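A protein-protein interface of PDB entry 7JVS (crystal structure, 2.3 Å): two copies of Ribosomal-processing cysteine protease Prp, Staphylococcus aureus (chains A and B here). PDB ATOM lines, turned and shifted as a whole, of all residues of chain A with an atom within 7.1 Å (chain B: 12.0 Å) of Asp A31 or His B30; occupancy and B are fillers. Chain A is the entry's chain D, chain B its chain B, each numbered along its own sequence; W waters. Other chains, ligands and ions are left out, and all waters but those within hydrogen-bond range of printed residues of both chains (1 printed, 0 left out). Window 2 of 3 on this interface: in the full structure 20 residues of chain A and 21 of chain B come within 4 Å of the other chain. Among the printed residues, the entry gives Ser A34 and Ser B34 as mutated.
Among the printed residues, merely in contact across the chains: Ile A32 with Ala B35 (3.3 Å), Ile A32 with Gly B29 (3.6 Å), Ala A35 with Ile B32 (3.7 Å), Gly A36 with Ala B39 (3.7 Å), Gly A36 with Ala B35 (3.7 Å), Ile A32 with Asp B31 (3.8 Å), Asp A31 with Ile B32 (3.9 Å) and Ile A32 with His B30 (3.9 Å).
Asp A31 touches His B30, but with the chains exchanged His A30 does not touch Asp B31 (9.3 Å). Ile A32 touches Gly B29, but with the chains exchanged Gly A29 does not touch Ile B32 (8.5 Å). Ile A32 touches Ala B35, and with the chains exchanged Ala A35 touches Ile B32. Gly A36 touches Ala B35, but with the chains exchanged Ala A35 does not touch Gly B36 (4.03 Å).
Of the 22 printed residues of chain B, 6 touch a printed residue of chain A. Hydrophobic or aromatic side chains of chain B that line the printed part of chain A: His B30, Ile B32, Ala B35 and Ala B39. Printed residues of chain A that touch a printed residue of chain B: Asp A31, Ile A32, Ala A35 and Gly A36. Hydrophobic or aromatic side chains of chain A within 4 Å of the printed part of chain B: Ile A32 and Ala A35. Among the printed residues, no Asp or Glu carboxylate lies within 4 Å of a Lys or Arg side-chain nitrogen of the other chain.
No residue of chain B comes within 4 Å of Tyr A28. No residue of chain B comes within 4 Å of Gly A29. No residue of chain B comes within 4 Å of His A30. Of chain B, only His B30 (2.7 Å) and Ile B32 (3.9 Å) come within 4 Å of Asp A31. Of chain B, only Gly B29 (3.6 Å), His B30 (3.9 Å), Asp B31 (3.8 Å) and Ala B35 (3.3 Å) come within 4 Å of Ile A32. No residue of chain B comes within 4 Å of Ser A34. Of chain B, only Ile B32 (3.7 Å) comes within 4 Å of Ala A35. Of the printed residues of chain B, Gly A36 touches Ala B35 (3.7 Å) and Ala B39 (3.7 Å). His B30 touches just these residues of chain A: Asp A31 (2.7 Å) and Ile A32 (3.9 Å). Of the printed residues of chain A, Asp B31 touches Ile A32. Of the printed residues of chain A, Ile B32 touches Asp A31 (3.9 Å) and Ala A35 (3.7 Å). The nearest residue of chain A that does not touch His B30 is Tyr A28 (4.3 Å). The nearest printed residue of chain B that does not touch Gly A36 is Gly B36 (4.4 Å).
N of His B25 lies within hydrogen-bond range of OD2 of Asp B31 (3.2 Å). OD2 of Asp B31 sits at hydrogen-bond distance from N of Gly B26 (3.4 Å). The backbone NH (N) of Val B33 is in hydrogen-bond range of the side-chain carboxylate (OD1) of Asp B31 (3.4 Å). The backbone NH of Ser B34 is in hydrogen-bond range of the side-chain carboxylate of Asp B31.
A ring nitrogen (ND1) of His B30 lies within hydrogen-bond range of the side-chain carboxylate (OD2) of Asp A31, at 2.7 Å.
Water W1 lies within hydrogen-bond range of the backbone carbonyl oxygen of His B30 and the side-chain carboxylate of Asp A31.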
ATOM      1  N   ILE A   2      13.072  32.437  19.616  1.00  0.00           N
ATOM      2  CA  ILE A   2      13.537  33.805  19.461  1.00  0.00           C
ATOM      3  C   ILE A   2      12.741  34.391  18.316  1.00  0.00           C
ATOM      4  O   ILE A   2      12.654  33.765  17.265  1.00  0.00           O
ATOM      5  CB  ILE A   2      15.018  33.841  19.085  1.00  0.00           C
ATOM      6  CG1 ILE A   2      15.841  33.212  20.212  1.00  0.00           C
ATOM      7  CG2 ILE A   2      15.464  35.272  18.806  1.00  0.00           C
ATOM      8  CD1 ILE A   2      16.708  32.084  19.744  1.00  0.00           C
ATOM      9  N   HIS A  25      13.040  30.174  28.278  1.00  0.00           N
ATOM     10  CA  HIS A  25      13.279  28.751  28.305  1.00  0.00           C
ATOM     11  C   HIS A  25      13.798  28.128  27.046  1.00  0.00           C
ATOM     12  O   HIS A  25      14.932  27.724  27.046  1.00  0.00           O
ATOM     13  CB  HIS A  25      12.018  28.000  28.785  1.00  0.00           C
ATOM     14  CG  HIS A  25      12.077  26.517  28.611  1.00  0.00           C
ATOM     15  ND1 HIS A  25      13.203  25.790  28.885  1.00  0.00           N
ATOM     16  CD2 HIS A  25      11.190  25.651  28.090  1.00  0.00           C
ATOM     17  CE1 HIS A  25      12.990  24.525  28.594  1.00  0.00           C
ATOM     18  NE2 HIS A  25      11.775  24.413  28.109  1.00  0.00           N
ATOM     19  N   GLY A  26      13.026  28.083  25.979  1.00  0.00           N
ATOM     20  CA  GLY A  26      13.429  27.419  24.760  1.00  0.00           C
ATOM     21  C   GLY A  26      13.624  25.909  24.696  1.00  0.00           C
ATOM     22  O   GLY A  26      13.958  25.253  25.619  1.00  0.00           O
ATOM     23  N   GLU A  27      13.474  25.354  23.529  1.00  0.00           N
ATOM     24  CA  GLU A  27      13.618  23.965  23.247  1.00  0.00           C
ATOM     25  C   GLU A  27      15.061  23.601  22.879  1.00  0.00           C
ATOM     26  O   GLU A  27      15.921  24.378  23.054  1.00  0.00           O
ATOM     27  CB  GLU A  27      12.687  23.679  22.087  1.00  0.00           C
ATOM     28  N   TYR A  28      15.309  22.360  22.514  1.00  0.00           N
ATOM     29  CA  TYR A  28      16.568  21.903  22.022  1.00  0.00           C
ATOM     30  C   TYR A  28      17.049  22.793  20.911  1.00  0.00           C
ATOM     31  O   TYR A  28      16.345  23.030  19.989  1.00  0.00           O
ATOM     32  CB  TYR A  28      16.394  20.496  21.469  1.00  0.00           C
ATOM     33  CG  TYR A  28      17.649  19.909  21.019  1.00  0.00           C
ATOM     34  CD1 TYR A  28      18.523  19.390  21.899  1.00  0.00           C
ATOM     35  CD2 TYR A  28      17.981  19.920  19.718  1.00  0.00           C
ATOM     36  CE1 TYR A  28      19.691  18.885  21.483  1.00  0.00           C
ATOM     37  CE2 TYR A  28      19.142  19.432  19.298  1.00  0.00           C
ATOM     38  CZ  TYR A  28      19.979  18.918  20.186  1.00  0.00           C
ATOM     39  OH  TYR A  28      21.141  18.455  19.747  1.00  0.00           O
ATOM     40  N   GLY A  29      18.215  23.360  21.020  1.00  0.00           N
ATOM     41  CA  GLY A  29      18.681  24.220  19.970  1.00  0.00           C
ATOM     42  C   GLY A  29      18.732  25.645  20.375  1.00  0.00           C
ATOM     43  O   GLY A  29      19.490  26.378  19.868  1.00  0.00           O
ATOM     44  N   HIS A  30      17.947  26.021  21.361  1.00  0.00           N
ATOM     45  CA  HIS A  30      17.861  27.375  21.826  1.00  0.00           C
ATOM     46  C   HIS A  30      19.115  28.001  22.311  1.00  0.00           C
ATOM     47  O   HIS A  30      19.371  29.090  22.011  1.00  0.00           O
ATOM     48  CB  HIS A  30      16.853  27.459  22.936  1.00  0.00           C
ATOM     49  CG  HIS A  30      16.498  28.832  23.347  1.00  0.00           C
ATOM     50  ND1 HIS A  30      15.809  29.685  22.546  1.00  0.00           N
ATOM     51  CD2 HIS A  30      16.691  29.481  24.504  1.00  0.00           C
ATOM     52  CE1 HIS A  30      15.604  30.805  23.184  1.00  0.00           C
ATOM     53  NE2 HIS A  30      16.135  30.709  24.373  1.00  0.00           N
ATOM     54  N   ASP A  31      19.879  27.299  23.133  1.00  0.00           N
ATOM     55  CA  ASP A  31      21.096  27.878  23.692  1.00  0.00           C
ATOM     56  C   ASP A  31      22.080  28.390  22.643  1.00  0.00           C
ATOM     57  O   ASP A  31      22.671  29.455  22.819  1.00  0.00           O
ATOM     58  CB  ASP A  31      21.793  26.866  24.591  1.00  0.00           C
ATOM     59  CG  ASP A  31      21.882  25.505  23.959  1.00  0.00           C
ATOM     60  OD1 ASP A  31      21.387  25.341  22.823  1.00  0.00           O
ATOM     61  OD2 ASP A  31      22.445  24.590  24.593  1.00  0.00           O
ATOM     62  N   ILE A  32      22.262  27.646  21.556  1.00  0.00           N
ATOM     63  CA  ILE A  32      23.195  28.050  20.563  1.00  0.00           C
ATOM     64  C   ILE A  32      22.660  29.072  19.612  1.00  0.00           C
ATOM     65  O   ILE A  32      23.363  29.938  19.265  1.00  0.00           O
ATOM     66  CB  ILE A  32      23.805  26.870  19.808  1.00  0.00           C
ATOM     67  CG1 ILE A  32      22.773  25.911  19.279  1.00  0.00           C
ATOM     68  CG2 ILE A  32      24.728  26.118  20.715  1.00  0.00           C
ATOM     69  CD1 ILE A  32      23.350  24.890  18.383  1.00  0.00           C
ATOM     70  N   VAL A  33      21.412  28.948  19.232  1.00  0.00           N
ATOM     71  CA  VAL A  33      20.747  29.860  18.323  1.00  0.00           C
ATOM     72  C   VAL A  33      20.597  31.266  18.976  1.00  0.00           C
ATOM     73  O   VAL A  33      20.859  32.273  18.337  1.00  0.00           O
ATOM     74  CB  VAL A  33      19.395  29.296  17.843  1.00  0.00           C
ATOM     75  CG1 VAL A  33      18.616  30.327  17.021  1.00  0.00           C
ATOM     76  CG2 VAL A  33      19.619  28.035  17.028  1.00  0.00           C
ATOM     77  N   SER A  34      20.214  31.304  20.255  1.00  0.00           N
ATOM     78  CA  SER A  34      20.218  32.537  21.057  1.00  0.00           C
ATOM     79  C   SER A  34      21.627  33.182  21.150  1.00  0.00           C
ATOM     80  O   SER A  34      21.772  34.401  21.042  1.00  0.00           O
ATOM     81  CB  SER A  34      19.648  32.254  22.458  1.00  0.00           C
ATOM     82  OG  SER A  34      19.898  33.318  23.356  1.00  0.00           O
ATOM     83  N   ALA A  35      22.648  32.344  21.353  1.00  0.00           N
ATOM     84  CA  ALA A  35      24.041  32.803  21.384  1.00  0.00           C
ATOM     85  C   ALA A  35      24.482  33.387  20.029  1.00  0.00           C
ATOM     86  O   ALA A  35      25.166  34.394  19.986  1.00  0.00           O
ATOM     87  CB  ALA A  35      24.969  31.657  21.787  1.00  0.00           C
ATOM     88  N   GLY A  36      24.080  32.733  18.933  1.00  0.00           N
ATOM     89  CA  GLY A  36      24.318  33.176  17.570  1.00  0.00           C
ATOM     90  C   GLY A  36      23.696  34.527  17.265  1.00  0.00           C
ATOM     91  O   GLY A  36      24.389  35.442  16.833  1.00  0.00           O
ATOM     92  N   ASN A 100      13.859  27.398  15.921  1.00  0.00           N
ATOM     93  CA  ASN A 100      14.285  28.195  17.074  1.00  0.00           C
ATOM     94  C   ASN A 100      14.266  29.714  16.905  1.00  0.00           C
ATOM     95  O   ASN A 100      14.376  30.448  17.888  1.00  0.00           O
ATOM     96  CB  ASN A 100      15.691  27.767  17.504  1.00  0.00           C
ATOM     97  CG  ASN A 100      15.789  26.280  17.778  1.00  0.00           C
ATOM     98  OD1 ASN A 100      16.325  25.521  16.969  1.00  0.00           O
ATOM     99  ND2 ASN A 100      15.272  25.853  18.924  1.00  0.00           N
ATOM    100  N   ILE B   2      39.905  29.233  19.648  1.00  0.00           N
ATOM    101  CA  ILE B   2      39.880  29.741  18.296  1.00  0.00           C
ATOM    102  C   ILE B   2      40.823  30.920  18.229  1.00  0.00           C
ATOM    103  O   ILE B   2      40.734  31.819  19.051  1.00  0.00           O
ATOM    104  CB  ILE B   2      38.481  30.233  17.921  1.00  0.00           C
ATOM    105  CG1 ILE B   2      37.461  29.101  18.072  1.00  0.00           C
ATOM    106  CG2 ILE B   2      38.473  30.799  16.505  1.00  0.00           C
ATOM    107  CD1 ILE B   2      36.090  29.606  18.448  1.00  0.00           C
ATOM    108  N   HIS B  22      39.085  25.256  17.720  1.00  0.00           N
ATOM    109  CA  HIS B  22      37.793  25.047  18.340  1.00  0.00           C
ATOM    110  C   HIS B  22      37.785  25.809  19.659  1.00  0.00           C
ATOM    111  O   HIS B  22      38.855  26.052  20.246  1.00  0.00           O
ATOM    112  CB  HIS B  22      37.542  23.554  18.575  1.00  0.00           C
ATOM    113  CG  HIS B  22      37.613  22.728  17.324  1.00  0.00           C
ATOM    114  ND1 HIS B  22      36.551  22.590  16.462  1.00  0.00           N
ATOM    115  CD2 HIS B  22      38.614  21.975  16.809  1.00  0.00           C
ATOM    116  CE1 HIS B  22      36.891  21.791  15.469  1.00  0.00           C
ATOM    117  NE2 HIS B  22      38.140  21.406  15.654  1.00  0.00           N
ATOM    118  N   ALA B  23      36.594  26.223  20.108  1.00  0.00           N
ATOM    119  CA  ALA B  23      36.451  27.141  21.248  1.00  0.00           C
ATOM    120  C   ALA B  23      36.672  26.464  22.596  1.00  0.00           C
ATOM    121  O   ALA B  23      37.192  27.080  23.534  1.00  0.00           O
ATOM    122  CB  ALA B  23      35.076  27.796  21.222  1.00  0.00           C
ATOM    123  N   ASP B  24      36.313  25.181  22.652  1.00  0.00           N
ATOM    124  CA  ASP B  24      36.442  24.347  23.849  1.00  0.00           C
ATOM    125  C   ASP B  24      35.786  24.988  25.068  1.00  0.00           C
ATOM    126  O   ASP B  24      36.362  25.017  26.155  1.00  0.00           O
ATOM    127  CB  ASP B  24      37.910  24.009  24.140  1.00  0.00           C
ATOM    128  CG  ASP B  24      38.579  23.276  22.993  1.00  0.00           C
ATOM    129  OD1 ASP B  24      37.882  22.526  22.278  1.00  0.00           O
ATOM    130  OD2 ASP B  24      39.802  23.451  22.808  1.00  0.00           O
ATOM    131  N   HIS B  25      34.574  25.498  24.874  1.00  0.00           N
ATOM    132  CA  HIS B  25      33.820  26.120  25.954  1.00  0.00           C
ATOM    133  C   HIS B  25      32.872  25.100  26.582  1.00  0.00           C
ATOM    134  O   HIS B  25      32.819  24.958  27.804  1.00  0.00           O
ATOM    135  CB  HIS B  25      33.034  27.325  25.434  1.00  0.00           C
ATOM    136  CG  HIS B  25      32.516  28.222  26.516  1.00  0.00           C
ATOM    137  ND1 HIS B  25      33.338  29.037  27.264  1.00  0.00           N
ATOM    138  CD2 HIS B  25      31.260  28.431  26.975  1.00  0.00           C
ATOM    139  CE1 HIS B  25      32.610  29.711  28.136  1.00  0.00           C
ATOM    140  NE2 HIS B  25      31.346  29.362  27.982  1.00  0.00           N
ATOM    141  N   GLY B  26      32.091  24.432  25.771  1.00  0.00           N
ATOM    142  CA  GLY B  26      31.144  23.465  26.221  1.00  0.00           C
ATOM    143  C   GLY B  26      31.222  22.194  25.408  1.00  0.00           C
ATOM    144  O   GLY B  26      32.217  21.908  24.804  1.00  0.00           O
ATOM    145  N   GLU B  27      30.150  21.431  25.414  1.00  0.00           N
ATOM    146  CA  GLU B  27      30.016  20.176  24.744  1.00  0.00           C
ATOM    147  C   GLU B  27      29.583  20.390  23.329  1.00  0.00           C
ATOM    148  O   GLU B  27      28.974  21.375  23.041  1.00  0.00           O
ATOM    149  CB  GLU B  27      29.021  19.273  25.477  1.00  0.00           C
ATOM    150  N   TYR B  28      29.909  19.482  22.426  1.00  0.00           N
ATOM    151  CA  TYR B  28      29.507  19.616  21.051  1.00  0.00           C
ATOM    152  C   TYR B  28      28.016  19.677  20.961  1.00  0.00           C
ATOM    153  O   TYR B  28      27.357  18.851  21.447  1.00  0.00           O
ATOM    154  CB  TYR B  28      29.991  18.488  20.178  1.00  0.00           C
ATOM    155  CG  TYR B  28      29.696  18.700  18.736  1.00  0.00           C
ATOM    156  CD1 TYR B  28      28.532  18.285  18.189  1.00  0.00           C
ATOM    157  CD2 TYR B  28      30.571  19.332  17.948  1.00  0.00           C
ATOM    158  CE1 TYR B  28      28.253  18.495  16.873  1.00  0.00           C
ATOM    159  CE2 TYR B  28      30.321  19.547  16.628  1.00  0.00           C
ATOM    160  CZ  TYR B  28      29.157  19.125  16.093  1.00  0.00           C
ATOM    161  OH  TYR B  28      28.928  19.332  14.795  1.00  0.00           O
ATOM    162  N   GLY B  29      27.468  20.730  20.364  1.00  0.00           N
ATOM    163  CA  GLY B  29      26.056  20.911  20.256  1.00  0.00           C
ATOM    164  C   GLY B  29      25.593  22.041  21.118  1.00  0.00           C
ATOM    165  O   GLY B  29      24.572  22.574  20.858  1.00  0.00           O
ATOM    166  N   HIS B  30      26.344  22.362  22.167  1.00  0.00           N
ATOM    167  CA  HIS B  30      26.025  23.372  23.145  1.00  0.00           C
ATOM    168  C   HIS B  30      27.145  24.358  23.447  1.00  0.00           C
ATOM    169  O   HIS B  30      27.194  24.901  24.508  1.00  0.00           O
ATOM    170  CB  HIS B  30      25.653  22.683  24.455  1.00  0.00           C
ATOM    171  CG  HIS B  30      24.569  21.675  24.298  1.00  0.00           C
ATOM    172  ND1 HIS B  30      23.254  22.030  24.161  1.00  0.00           N
ATOM    173  CD2 HIS B  30      24.623  20.343  24.093  1.00  0.00           C
ATOM    174  CE1 HIS B  30      22.535  20.952  23.952  1.00  0.00           C
ATOM    175  NE2 HIS B  30      23.342  19.915  23.909  1.00  0.00           N
ATOM    176  N   ASP B  31      28.032  24.588  22.509  1.00  0.00           N
ATOM    177  CA  ASP B  31      29.113  25.497  22.725  1.00  0.00           C
ATOM    178  C   ASP B  31      28.613  26.852  22.239  1.00  0.00           C
ATOM    179  O   ASP B  31      28.367  26.999  21.082  1.00  0.00           O
ATOM    180  CB  ASP B  31      30.315  25.026  21.930  1.00  0.00           C
ATOM    181  CG  ASP B  31      31.567  25.720  22.302  1.00  0.00           C
ATOM    182  OD1 ASP B  31      31.591  26.927  22.507  1.00  0.00           O
ATOM    183  OD2 ASP B  31      32.549  25.030  22.407  1.00  0.00           O
ATOM    184  N   ILE B  32      28.478  27.826  23.121  1.00  0.00           N
ATOM    185  CA  ILE B  32      27.944  29.128  22.775  1.00  0.00           C
ATOM    186  C   ILE B  32      28.928  30.083  22.110  1.00  0.00           C
ATOM    187  O   ILE B  32      28.542  30.889  21.332  1.00  0.00           O
ATOM    188  CB  ILE B  32      27.281  29.791  23.981  1.00  0.00           C
ATOM    189  CG1 ILE B  32      28.273  30.012  25.087  1.00  0.00           C
ATOM    190  CG2 ILE B  32      26.139  28.946  24.491  1.00  0.00           C
ATOM    191  CD1 ILE B  32      27.647  30.518  26.336  1.00  0.00           C
ATOM    192  N   VAL B  33      30.184  29.989  22.467  1.00  0.00           N
ATOM    193  CA  VAL B  33      31.268  30.761  21.866  1.00  0.00           C
ATOM    194  C   VAL B  33      31.429  30.406  20.373  1.00  0.00           C
ATOM    195  O   VAL B  33      31.534  31.299  19.524  1.00  0.00           O
ATOM    196  CB  VAL B  33      32.591  30.540  22.644  1.00  0.00           C
ATOM    197  CG1 VAL B  33      33.770  31.197  21.935  1.00  0.00           C
ATOM    198  CG2 VAL B  33      32.467  31.053  24.077  1.00  0.00           C
ATOM    199  N   SER B  34      31.440  29.098  20.072  1.00  0.00           N
ATOM    200  CA  SER B  34      31.426  28.595  18.691  1.00  0.00           C
ATOM    201  C   SER B  34      30.178  29.053  17.923  1.00  0.00           C
ATOM    202  O   SER B  34      30.253  29.417  16.748  1.00  0.00           O
ATOM    203  CB  SER B  34      31.541  27.055  18.667  1.00  0.00           C
ATOM    204  OG  SER B  34      31.181  26.506  17.405  1.00  0.00           O
ATOM    205  N   ALA B  35      29.014  29.028  18.579  1.00  0.00           N
ATOM    206  CA  ALA B  35      27.765  29.508  17.971  1.00  0.00           C
ATOM    207  C   ALA B  35      27.851  31.009  17.626  1.00  0.00           C
ATOM    208  O   ALA B  35      27.431  31.413  16.546  1.00  0.00           O
ATOM    209  CB  ALA B  35      26.591  29.233  18.879  1.00  0.00           C
ATOM    210  N   GLY B  36      28.418  31.802  18.547  1.00  0.00           N
ATOM    211  CA  GLY B  36      28.653  33.224  18.350  1.00  0.00           C
ATOM    212  C   GLY B  36      29.573  33.523  17.152  1.00  0.00           C
ATOM    213  O   GLY B  36      29.203  34.273  16.237  1.00  0.00           O
ATOM    214  N   ALA B  37      30.773  32.929  17.164  1.00  0.00           N
ATOM    215  CA  ALA B  37      31.778  33.198  16.130  1.00  0.00           C
ATOM    216  C   ALA B  37      31.330  32.702  14.761  1.00  0.00           C
ATOM    217  O   ALA B  37      31.535  33.395  13.756  1.00  0.00           O
ATOM    218  CB  ALA B  37      33.114  32.615  16.500  1.00  0.00           C
ATOM    219  N   SER B  38      30.681  31.531  14.742  1.00  0.00           N
ATOM    220  CA  SER B  38      30.195  30.934  13.508  1.00  0.00           C
ATOM    221  C   SER B  38      29.130  31.808  12.860  1.00  0.00           C
ATOM    222  O   SER B  38      29.235  32.130  11.666  1.00  0.00           O
ATOM    223  CB  SER B  38      29.661  29.511  13.761  1.00  0.00           C
ATOM    224  OG  SER B  38      30.695  28.662  14.277  1.00  0.00           O
ATOM    225  N   ALA B  39      28.121  32.207  13.648  1.00  0.00           N
ATOM    226  CA  ALA B  39      27.022  33.037  13.145  1.00  0.00           C
ATOM    227  C   ALA B  39      27.541  34.341  12.538  1.00  0.00           C
ATOM    228  O   ALA B  39      27.040  34.801  11.509  1.00  0.00           O
ATOM    229  CB  ALA B  39      26.009  33.337  14.230  1.00  0.00           C
ATOM    230  N   ILE B  93      33.062  39.273  21.369  1.00  0.00           N
ATOM    231  CA  ILE B  93      33.086  37.926  21.936  1.00  0.00           C
ATOM    232  C   ILE B  93      34.394  37.693  22.718  1.00  0.00           C
ATOM    233  O   ILE B  93      34.356  37.180  23.824  1.00  0.00           O
ATOM    234  CB  ILE B  93      32.864  36.835  20.864  1.00  0.00           C
ATOM    235  CG1 ILE B  93      31.527  37.036  20.146  1.00  0.00           C
ATOM    236  CG2 ILE B  93      32.867  35.451  21.500  1.00  0.00           C
ATOM    237  CD1 ILE B  93      31.384  36.221  18.875  1.00  0.00           C
ATOM    238  N   TYR B  97      34.793  36.356  26.535  1.00  0.00           N
ATOM    239  CA  TYR B  97      35.220  34.986  26.611  1.00  0.00           C
ATOM    240  C   TYR B  97      36.657  34.929  26.217  1.00  0.00           C
ATOM    241  O   TYR B  97      37.015  34.347  25.231  1.00  0.00           O
ATOM    242  CB  TYR B  97      34.404  34.109  25.701  1.00  0.00           C
ATOM    243  CG  TYR B  97      32.992  34.020  26.120  1.00  0.00           C
ATOM    244  CD1 TYR B  97      32.596  33.140  27.060  1.00  0.00           C
ATOM    245  CD2 TYR B  97      32.060  34.826  25.580  1.00  0.00           C
ATOM    246  CE1 TYR B  97      31.313  33.073  27.449  1.00  0.00           C
ATOM    247  CE2 TYR B  97      30.774  34.774  25.976  1.00  0.00           C
ATOM    248  CZ  TYR B  97      30.407  33.885  26.898  1.00  0.00           C
ATOM    249  OH  TYR B  97      29.118  33.843  27.262  1.00  0.00           O
ATOM    250  N   ASN B 100      38.598  31.647  25.154  1.00  0.00           N
ATOM    251  CA  ASN B 100      38.077  30.819  24.070  1.00  0.00           C
ATOM    252  C   ASN B 100      38.406  31.342  22.659  1.00  0.00           C
ATOM    253  O   ASN B 100      38.453  30.560  21.709  1.00  0.00           O
ATOM    254  CB  ASN B 100      36.560  30.665  24.214  1.00  0.00           C
ATOM    255  CG  ASN B 100      36.161  30.045  25.537  1.00  0.00           C
ATOM    256  OD1 ASN B 100      35.520  30.689  26.368  1.00  0.00           O
ATOM    257  ND2 ASN B 100      36.539  28.788  25.740  1.00  0.00           N
HETATM  258  O   HOH W   1      25.069  25.494  26.053  1.00  0.00           O
